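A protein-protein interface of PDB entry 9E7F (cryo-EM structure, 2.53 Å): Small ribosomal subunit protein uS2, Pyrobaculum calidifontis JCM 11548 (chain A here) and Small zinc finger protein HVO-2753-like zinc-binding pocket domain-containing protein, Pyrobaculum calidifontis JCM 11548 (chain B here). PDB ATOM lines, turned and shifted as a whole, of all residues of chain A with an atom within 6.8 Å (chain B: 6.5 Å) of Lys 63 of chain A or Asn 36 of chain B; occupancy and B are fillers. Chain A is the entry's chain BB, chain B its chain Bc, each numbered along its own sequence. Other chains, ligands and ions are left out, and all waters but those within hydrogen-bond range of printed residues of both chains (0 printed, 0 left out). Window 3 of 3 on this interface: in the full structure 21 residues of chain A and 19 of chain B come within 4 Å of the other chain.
The side-chain amino group (NZ) of Lys 63 of chain A is in hydrogen-bond range of the side-chain amide oxygen (OD1) of Asn 36 of chain B, 2.8 Å away.
The guanidinium group of Arg 67 of chain A is in hydrogen-bond range of the backbone carbonyl oxygen of Cys 34 of chain B, 2.7 Å away.
The guanidinium group (NH2) of Arg 67 of chain A lies close to the backbone carbonyl oxygen (O) of Pro 35 of chain B, 3.2 Å away.
The guanidinium group (NH1) of Arg 67 of chain A sits at hydrogen-bond distance from the backbone carbonyl oxygen (O) of Cys 37 of chain B, at 3.4 Å.
NH1 of Arg 67 of chain A sits close to N of Gly 38 of chain B (3.4 Å).
SG of Cys 34 of chain B sits close to N of Asn 36 of chain B, at 3.4 Å.
The side-chain sulfur (SG) of Cys 37 of chain B lies close to the side-chain amide nitrogen (ND2) of Asn 36 of chain B, at 3.0 Å.
ND2 of Asn 36 of chain B sits close to SG of Cys 60 of chain B, at 2.8 Å.
N of Cys 57 of chain B sits at hydrogen-bond distance from O of Phe 62 of chain B, at 2.9 Å.
SG of Cys 60 of chain B sits close to N of Phe 62 of chain B (3.3 Å).
Among the printed residues, merely in contact across the chains: Ile 60 of chain A with Pro 35 of chain B (3.3 Å), Phe 158 of chain A with Phe 62 of chain B (3.4 Å), Ile 60 of chain A with Asn 36 of chain B (3.5 Å), Lys 63 of chain A with Pro 35 of chain B (3.6 Å) and Ile 60 of chain A with Phe 62 of chain B (3.8 Å).
Ala 62 of chain A touches none of the printed residues of chain B.
Lys 63 of chain A touches two residues of chain B.
Printed residues of chain A within 4 Å of Cys 34 of chain B: Arg 67.
Asn 36 of chain B touches two residues of chain A.
Printed residues of chain A within 4 Å of Gly 38 of chain B: Arg 67 (3.3 Å).
The nearest residue of chain B that does not touch Lys 63 of chain A is Cys 37 of chain B (4.8 Å).
The nearest residue of chain A that does not touch Asn 36 of chain B is Arg 67 of chain A (4.1 Å).
Of the 17 printed residues of chain A, 4 touch a printed residue of chain B.
Hydrophobic or aromatic side chains of chain B that line the printed part of chain A: Pro 35 and Phe 62.
Along chain B the printed residues that touch a printed residue of chain A span positions 34 to 62.
Among the printed residues, no Asp or Glu carboxylate lies within 4 Å of a Lys or Arg side-chain nitrogen of the other chain.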
ATOM      1  N   GLU A  56      -5.306  25.012  27.399  1.00  0.00           N
ATOM      2  CA  GLU A  56      -4.693  23.826  26.814  1.00  0.00           C
ATOM      3  C   GLU A  56      -5.276  23.524  25.444  1.00  0.00           C
ATOM      4  O   GLU A  56      -4.558  23.102  24.533  1.00  0.00           O
ATOM      5  CB  GLU A  56      -4.874  22.637  27.749  1.00  0.00           C
ATOM      6  CG  GLU A  56      -4.228  21.370  27.257  1.00  0.00           C
ATOM      7  CD  GLU A  56      -5.246  20.390  26.721  1.00  0.00           C
ATOM      8  OE1 GLU A  56      -6.362  20.830  26.375  1.00  0.00           O
ATOM      9  OE2 GLU A  56      -4.936  19.183  26.647  1.00  0.00           O
ATOM     10  N   LEU A  58      -6.549  25.774  23.401  1.00  0.00           N
ATOM     11  CA  LEU A  58      -6.097  26.800  22.467  1.00  0.00           C
ATOM     12  C   LEU A  58      -4.749  26.437  21.860  1.00  0.00           C
ATOM     13  O   LEU A  58      -4.537  26.608  20.655  1.00  0.00           O
ATOM     14  CB  LEU A  58      -6.016  28.156  23.165  1.00  0.00           C
ATOM     15  CG  LEU A  58      -7.301  28.681  23.799  1.00  0.00           C
ATOM     16  CD1 LEU A  58      -7.202  30.165  24.059  1.00  0.00           C
ATOM     17  CD2 LEU A  58      -8.479  28.382  22.909  1.00  0.00           C
ATOM     18  N   ARG A  59      -3.825  25.938  22.684  1.00  0.00           N
ATOM     19  CA  ARG A  59      -2.501  25.566  22.193  1.00  0.00           C
ATOM     20  C   ARG A  59      -2.587  24.420  21.197  1.00  0.00           C
ATOM     21  O   ARG A  59      -1.943  24.447  20.144  1.00  0.00           O
ATOM     22  CB  ARG A  59      -1.600  25.180  23.365  1.00  0.00           C
ATOM     23  CG  ARG A  59      -1.476  26.245  24.431  1.00  0.00           C
ATOM     24  CD  ARG A  59      -0.672  25.746  25.612  1.00  0.00           C
ATOM     25  NE  ARG A  59      -0.755  26.655  26.747  1.00  0.00           N
ATOM     26  CZ  ARG A  59       0.285  27.270  27.290  1.00  0.00           C
ATOM     27  NH1 ARG A  59       1.511  27.086  26.834  1.00  0.00           N
ATOM     28  NH2 ARG A  59       0.089  28.091  28.317  1.00  0.00           N
ATOM     29  N   ILE A  60      -3.384  23.402  21.517  1.00  0.00           N
ATOM     30  CA  ILE A  60      -3.529  22.263  20.620  1.00  0.00           C
ATOM     31  C   ILE A  60      -4.225  22.675  19.339  1.00  0.00           C
ATOM     32  O   ILE A  60      -3.970  22.105  18.273  1.00  0.00           O
ATOM     33  CB  ILE A  60      -4.284  21.128  21.324  1.00  0.00           C
ATOM     34  CG1 ILE A  60      -3.665  20.856  22.691  1.00  0.00           C
ATOM     35  CG2 ILE A  60      -4.267  19.890  20.464  1.00  0.00           C
ATOM     36  CD1 ILE A  60      -4.436  19.868  23.509  1.00  0.00           C
ATOM     37  N   ALA A  61      -5.132  23.647  19.423  1.00  0.00           N
ATOM     38  CA  ALA A  61      -5.759  24.176  18.221  1.00  0.00           C
ATOM     39  C   ALA A  61      -4.727  24.838  17.320  1.00  0.00           C
ATOM     40  O   ALA A  61      -4.732  24.641  16.099  1.00  0.00           O
ATOM     41  CB  ALA A  61      -6.860  25.163  18.598  1.00  0.00           C
ATOM     42  N   ALA A  62      -3.821  25.618  17.914  1.00  0.00           N
ATOM     43  CA  ALA A  62      -2.748  26.232  17.142  1.00  0.00           C
ATOM     44  C   ALA A  62      -1.834  25.176  16.539  1.00  0.00           C
ATOM     45  O   ALA A  62      -1.343  25.337  15.415  1.00  0.00           O
ATOM     46  CB  ALA A  62      -1.951  27.189  18.023  1.00  0.00           C
ATOM     47  N   LYS A  63      -1.591  24.092  17.276  1.00  0.00           N
ATOM     48  CA  LYS A  63      -0.797  22.989  16.747  1.00  0.00           C
ATOM     49  C   LYS A  63      -1.475  22.360  15.539  1.00  0.00           C
ATOM     50  O   LYS A  63      -0.818  22.036  14.544  1.00  0.00           O
ATOM     51  CB  LYS A  63      -0.566  21.948  17.844  1.00  0.00           C
ATOM     52  CG  LYS A  63       0.733  22.126  18.612  1.00  0.00           C
ATOM     53  CD  LYS A  63       1.040  20.916  19.481  1.00  0.00           C
ATOM     54  CE  LYS A  63       0.561  21.117  20.911  1.00  0.00           C
ATOM     55  NZ  LYS A  63       0.493  19.844  21.685  1.00  0.00           N
ATOM     56  N   LEU A  64      -2.797  22.199  15.604  1.00  0.00           N
ATOM     57  CA  LEU A  64      -3.526  21.542  14.528  1.00  0.00           C
ATOM     58  C   LEU A  64      -3.568  22.420  13.284  1.00  0.00           C
ATOM     59  O   LEU A  64      -3.375  21.938  12.162  1.00  0.00           O
ATOM     60  CB  LEU A  64      -4.935  21.193  15.021  1.00  0.00           C
ATOM     61  CG  LEU A  64      -6.016  20.419  14.244  1.00  0.00           C
ATOM     62  CD1 LEU A  64      -6.505  21.061  12.953  1.00  0.00           C
ATOM     63  CD2 LEU A  64      -5.548  19.001  13.980  1.00  0.00           C
ATOM     64  N   ILE A  65      -3.828  23.717  13.466  1.00  0.00           N
ATOM     65  CA  ILE A  65      -3.938  24.636  12.337  1.00  0.00           C
ATOM     66  C   ILE A  65      -2.597  24.803  11.641  1.00  0.00           C
ATOM     67  O   ILE A  65      -2.535  24.921  10.412  1.00  0.00           O
ATOM     68  CB  ILE A  65      -4.498  25.989  12.804  1.00  0.00           C
ATOM     69  CG1 ILE A  65      -5.820  25.791  13.545  1.00  0.00           C
ATOM     70  CG2 ILE A  65      -4.654  26.934  11.632  1.00  0.00           C
ATOM     71  CD1 ILE A  65      -6.596  27.062  13.757  1.00  0.00           C
ATOM     72  N   ALA A  66      -1.506  24.818  12.408  1.00  0.00           N
ATOM     73  CA  ALA A  66      -0.188  25.059  11.834  1.00  0.00           C
ATOM     74  C   ALA A  66       0.259  23.943  10.901  1.00  0.00           C
ATOM     75  O   ALA A  66       1.132  24.171  10.058  1.00  0.00           O
ATOM     76  CB  ALA A  66       0.841  25.251  12.947  1.00  0.00           C
ATOM     77  N   ARG A  67      -0.320  22.753  11.017  1.00  0.00           N
ATOM     78  CA  ARG A  67       0.074  21.637  10.171  1.00  0.00           C
ATOM     79  C   ARG A  67      -0.628  21.629   8.822  1.00  0.00           C
ATOM     80  O   ARG A  67      -0.459  20.671   8.064  1.00  0.00           O
ATOM     81  CB  ARG A  67      -0.180  20.318  10.896  1.00  0.00           C
ATOM     82  CG  ARG A  67       0.687  20.158  12.124  1.00  0.00           C
ATOM     83  CD  ARG A  67       0.521  18.797  12.751  1.00  0.00           C
ATOM     84  NE  ARG A  67      -0.813  18.600  13.296  1.00  0.00           N
ATOM     85  CZ  ARG A  67      -1.066  18.331  14.567  1.00  0.00           C
ATOM     86  NH1 ARG A  67      -0.096  18.260  15.463  1.00  0.00           N
ATOM     87  NH2 ARG A  67      -2.321  18.129  14.948  1.00  0.00           N
ATOM     88  N   TYR A  68      -1.422  22.648   8.513  1.00  0.00           N
ATOM     89  CA  TYR A  68      -2.005  22.765   7.193  1.00  0.00           C
ATOM     90  C   TYR A  68      -1.471  24.018   6.519  1.00  0.00           C
ATOM     91  O   TYR A  68      -1.039  24.947   7.209  1.00  0.00           O
ATOM     92  CB  TYR A  68      -3.549  22.824   7.212  1.00  0.00           C
ATOM     93  CG  TYR A  68      -4.245  21.645   7.867  1.00  0.00           C
ATOM     94  CD1 TYR A  68      -4.252  21.481   9.246  1.00  0.00           C
ATOM     95  CD2 TYR A  68      -4.866  20.674   7.096  1.00  0.00           C
ATOM     96  CE1 TYR A  68      -4.865  20.406   9.832  1.00  0.00           C
ATOM     97  CE2 TYR A  68      -5.484  19.592   7.679  1.00  0.00           C
ATOM     98  CZ  TYR A  68      -5.479  19.465   9.044  1.00  0.00           C
ATOM     99  OH  TYR A  68      -6.093  18.388   9.628  1.00  0.00           O
ATOM    100  N   PHE A 158     -12.706  18.747  16.531  1.00  0.00           N
ATOM    101  CA  PHE A 158     -12.032  19.400  17.640  1.00  0.00           C
ATOM    102  C   PHE A 158     -12.901  20.542  18.137  1.00  0.00           C
ATOM    103  O   PHE A 158     -13.416  21.326  17.340  1.00  0.00           O
ATOM    104  CB  PHE A 158     -10.656  19.928  17.235  1.00  0.00           C
ATOM    105  CG  PHE A 158      -9.803  20.325  18.399  1.00  0.00           C
ATOM    106  CD1 PHE A 158      -9.048  19.385  19.067  1.00  0.00           C
ATOM    107  CD2 PHE A 158      -9.772  21.632  18.839  1.00  0.00           C
ATOM    108  CE1 PHE A 158      -8.269  19.747  20.141  1.00  0.00           C
ATOM    109  CE2 PHE A 158      -8.994  21.995  19.915  1.00  0.00           C
ATOM    110  CZ  PHE A 158      -8.243  21.050  20.565  1.00  0.00           C
ATOM    111  N   LEU A 177      -5.182  32.824  19.648  1.00  0.00           N
ATOM    112  CA  LEU A 177      -5.053  31.757  18.668  1.00  0.00           C
ATOM    113  C   LEU A 177      -4.275  32.221  17.443  1.00  0.00           C
ATOM    114  O   LEU A 177      -3.510  31.448  16.857  1.00  0.00           O
ATOM    115  CB  LEU A 177      -6.437  31.250  18.273  1.00  0.00           C
ATOM    116  CG  LEU A 177      -6.498  29.800  17.801  1.00  0.00           C
ATOM    117  CD1 LEU A 177      -5.981  28.867  18.872  1.00  0.00           C
ATOM    118  CD2 LEU A 177      -7.907  29.428  17.391  1.00  0.00           C
ATOM    119  N   GLN A 180      -0.562  32.240  18.604  1.00  0.00           N
ATOM    120  CA  GLN A 180       0.060  30.949  18.871  1.00  0.00           C
ATOM    121  C   GLN A 180       0.358  30.188  17.587  1.00  0.00           C
ATOM    122  O   GLN A 180       1.351  29.456  17.512  1.00  0.00           O
ATOM    123  CB  GLN A 180      -0.835  30.115  19.779  1.00  0.00           C
ATOM    124  CG  GLN A 180      -0.149  28.901  20.360  1.00  0.00           C
ATOM    125  CD  GLN A 180       0.762  29.250  21.513  1.00  0.00           C
ATOM    126  OE1 GLN A 180       1.655  30.077  21.379  1.00  0.00           O
ATOM    127  NE2 GLN A 180       0.538  28.616  22.656  1.00  0.00           N
ATOM    128  N   VAL A 181      -0.491  30.335  16.571  1.00  0.00           N
ATOM    129  CA  VAL A 181      -0.271  29.603  15.327  1.00  0.00           C
ATOM    130  C   VAL A 181       0.971  30.124  14.620  1.00  0.00           C
ATOM    131  O   VAL A 181       1.663  29.377  13.921  1.00  0.00           O
ATOM    132  CB  VAL A 181      -1.522  29.665  14.428  1.00  0.00           C
ATOM    133  CG1 VAL A 181      -1.576  30.956  13.641  1.00  0.00           C
ATOM    134  CG2 VAL A 181      -1.555  28.477  13.492  1.00  0.00           C
ATOM    135  N   GLU A 184       4.053  28.515  16.498  1.00  0.00           N
ATOM    136  CA  GLU A 184       4.242  27.154  16.013  1.00  0.00           C
ATOM    137  C   GLU A 184       4.642  27.141  14.546  1.00  0.00           C
ATOM    138  O   GLU A 184       5.456  26.306  14.134  1.00  0.00           O
ATOM    139  CB  GLU A 184       2.978  26.329  16.236  1.00  0.00           C
ATOM    140  CG  GLU A 184       2.297  26.595  17.570  1.00  0.00           C
ATOM    141  CD  GLU A 184       2.351  25.407  18.509  1.00  0.00           C
ATOM    142  OE1 GLU A 184       2.824  24.332  18.089  1.00  0.00           O
ATOM    143  OE2 GLU A 184       1.915  25.549  19.671  1.00  0.00           O
ATOM    144  N   ALA B  33      -4.036  13.816  11.798  1.00  0.00           N
ATOM    145  CA  ALA B  33      -3.085  13.398  12.814  1.00  0.00           C
ATOM    146  C   ALA B  33      -3.590  13.808  14.188  1.00  0.00           C
ATOM    147  O   ALA B  33      -4.587  14.522  14.312  1.00  0.00           O
ATOM    148  CB  ALA B  33      -1.706  14.007  12.555  1.00  0.00           C
ATOM    149  N   CYS B  34      -2.904  13.340  15.223  1.00  0.00           N
ATOM    150  CA  CYS B  34      -3.272  13.708  16.579  1.00  0.00           C
ATOM    151  C   CYS B  34      -3.108  15.214  16.766  1.00  0.00           C
ATOM    152  O   CYS B  34      -2.092  15.776  16.335  1.00  0.00           O
ATOM    153  CB  CYS B  34      -2.418  12.962  17.602  1.00  0.00           C
ATOM    154  SG  CYS B  34      -2.668  13.540  19.298  1.00  0.00           S
ATOM    155  N   PRO B  35      -4.101  15.904  17.334  1.00  0.00           N
ATOM    156  CA  PRO B  35      -3.974  17.359  17.507  1.00  0.00           C
ATOM    157  C   PRO B  35      -2.815  17.760  18.394  1.00  0.00           C
ATOM    158  O   PRO B  35      -2.150  18.767  18.122  1.00  0.00           O
ATOM    159  CB  PRO B  35      -5.324  17.752  18.121  1.00  0.00           C
ATOM    160  CG  PRO B  35      -6.240  16.621  17.794  1.00  0.00           C
ATOM    161  CD  PRO B  35      -5.387  15.403  17.838  1.00  0.00           C
ATOM    162  N   ASN B  36      -2.534  16.980  19.436  1.00  0.00           N
ATOM    163  CA  ASN B  36      -1.426  17.312  20.320  1.00  0.00           C
ATOM    164  C   ASN B  36      -0.095  16.921  19.690  1.00  0.00           C
ATOM    165  O   ASN B  36       0.780  17.768  19.486  1.00  0.00           O
ATOM    166  CB  ASN B  36      -1.614  16.631  21.673  1.00  0.00           C
ATOM    167  CG  ASN B  36      -0.306  16.368  22.374  1.00  0.00           C
ATOM    168  OD1 ASN B  36       0.329  17.286  22.887  1.00  0.00           O
ATOM    169  ND2 ASN B  36       0.112  15.109  22.391  1.00  0.00           N
ATOM    170  N   CYS B  37       0.070  15.641  19.352  1.00  0.00           N
ATOM    171  CA  CYS B  37       1.320  15.200  18.747  1.00  0.00           C
ATOM    172  C   CYS B  37       1.375  15.566  17.275  1.00  0.00           C
ATOM    173  O   CYS B  37       2.268  16.295  16.837  1.00  0.00           O
ATOM    174  CB  CYS B  37       1.499  13.688  18.904  1.00  0.00           C
ATOM    175  SG  CYS B  37       0.921  12.993  20.447  1.00  0.00           S
ATOM    176  N   GLY B  38       0.413  15.082  16.504  1.00  0.00           N
ATOM    177  CA  GLY B  38       0.550  15.035  15.069  1.00  0.00           C
ATOM    178  C   GLY B  38       1.241  13.795  14.563  1.00  0.00           C
ATOM    179  O   GLY B  38       1.522  13.706  13.363  1.00  0.00           O
ATOM    180  N   LYS B  39       1.525  12.833  15.439  1.00  0.00           N
ATOM    181  CA  LYS B  39       2.237  11.621  15.056  1.00  0.00           C
ATOM    182  C   LYS B  39       1.287  10.538  14.560  1.00  0.00           C
ATOM    183  O   LYS B  39       1.376  10.103  13.408  1.00  0.00           O
ATOM    184  CB  LYS B  39       3.059  11.107  16.243  1.00  0.00           C
ATOM    185  CG  LYS B  39       3.929  12.166  16.892  1.00  0.00           C
ATOM    186  CD  LYS B  39       5.302  12.216  16.246  1.00  0.00           C
ATOM    187  CE  LYS B  39       6.282  13.010  17.089  1.00  0.00           C
ATOM    188  NZ  LYS B  39       6.536  12.360  18.401  1.00  0.00           N
ATOM    189  N   CYS B  57      -5.484   9.236  21.525  1.00  0.00           N
ATOM    190  CA  CYS B  57      -4.193   9.014  20.891  1.00  0.00           C
ATOM    191  C   CYS B  57      -3.545   7.768  21.479  1.00  0.00           C
ATOM    192  O   CYS B  57      -3.464   7.637  22.703  1.00  0.00           O
ATOM    193  CB  CYS B  57      -3.276  10.219  21.081  1.00  0.00           C
ATOM    194  SG  CYS B  57      -1.655  10.043  20.283  1.00  0.00           S
ATOM    195  N   CYS B  60      -0.012   9.646  22.955  1.00  0.00           N
ATOM    196  CA  CYS B  60      -0.212  10.578  24.052  1.00  0.00           C
ATOM    197  C   CYS B  60      -1.622  10.406  24.598  1.00  0.00           C
ATOM    198  O   CYS B  60      -2.477   9.775  23.977  1.00  0.00           O
ATOM    199  CB  CYS B  60       0.002  12.027  23.610  1.00  0.00           C
ATOM    200  SG  CYS B  60      -1.473  12.809  22.937  1.00  0.00           S
ATOM    201  N   GLY B  61      -1.873  10.995  25.760  1.00  0.00           N
ATOM    202  CA  GLY B  61      -3.137  10.750  26.420  1.00  0.00           C
ATOM    203  C   GLY B  61      -4.292  11.608  25.952  1.00  0.00           C
ATOM    204  O   GLY B  61      -5.344  11.624  26.599  1.00  0.00           O
ATOM    205  N   PHE B  62      -4.130  12.302  24.827  1.00  0.00           N
ATOM    206  CA  PHE B  62      -5.147  13.234  24.361  1.00  0.00           C
ATOM    207  C   PHE B  62      -6.392  12.485  23.913  1.00  0.00           C
ATOM    208  O   PHE B  62      -6.305  11.483  23.196  1.00  0.00           O
ATOM    209  CB  PHE B  62      -4.609  14.092  23.218  1.00  0.00           C
ATOM    210  CG  PHE B  62      -5.628  15.019  22.616  1.00  0.00           C
ATOM    211  CD1 PHE B  62      -6.278  14.691  21.438  1.00  0.00           C
ATOM    212  CD2 PHE B  62      -5.928  16.220  23.220  1.00  0.00           C
ATOM    213  CE1 PHE B  62      -7.212  15.535  20.888  1.00  0.00           C
ATOM    214  CE2 PHE B  62      -6.858  17.071  22.666  1.00  0.00           C
ATOM    215  CZ  PHE B  62      -7.501  16.723  21.499  1.00  0.00           C
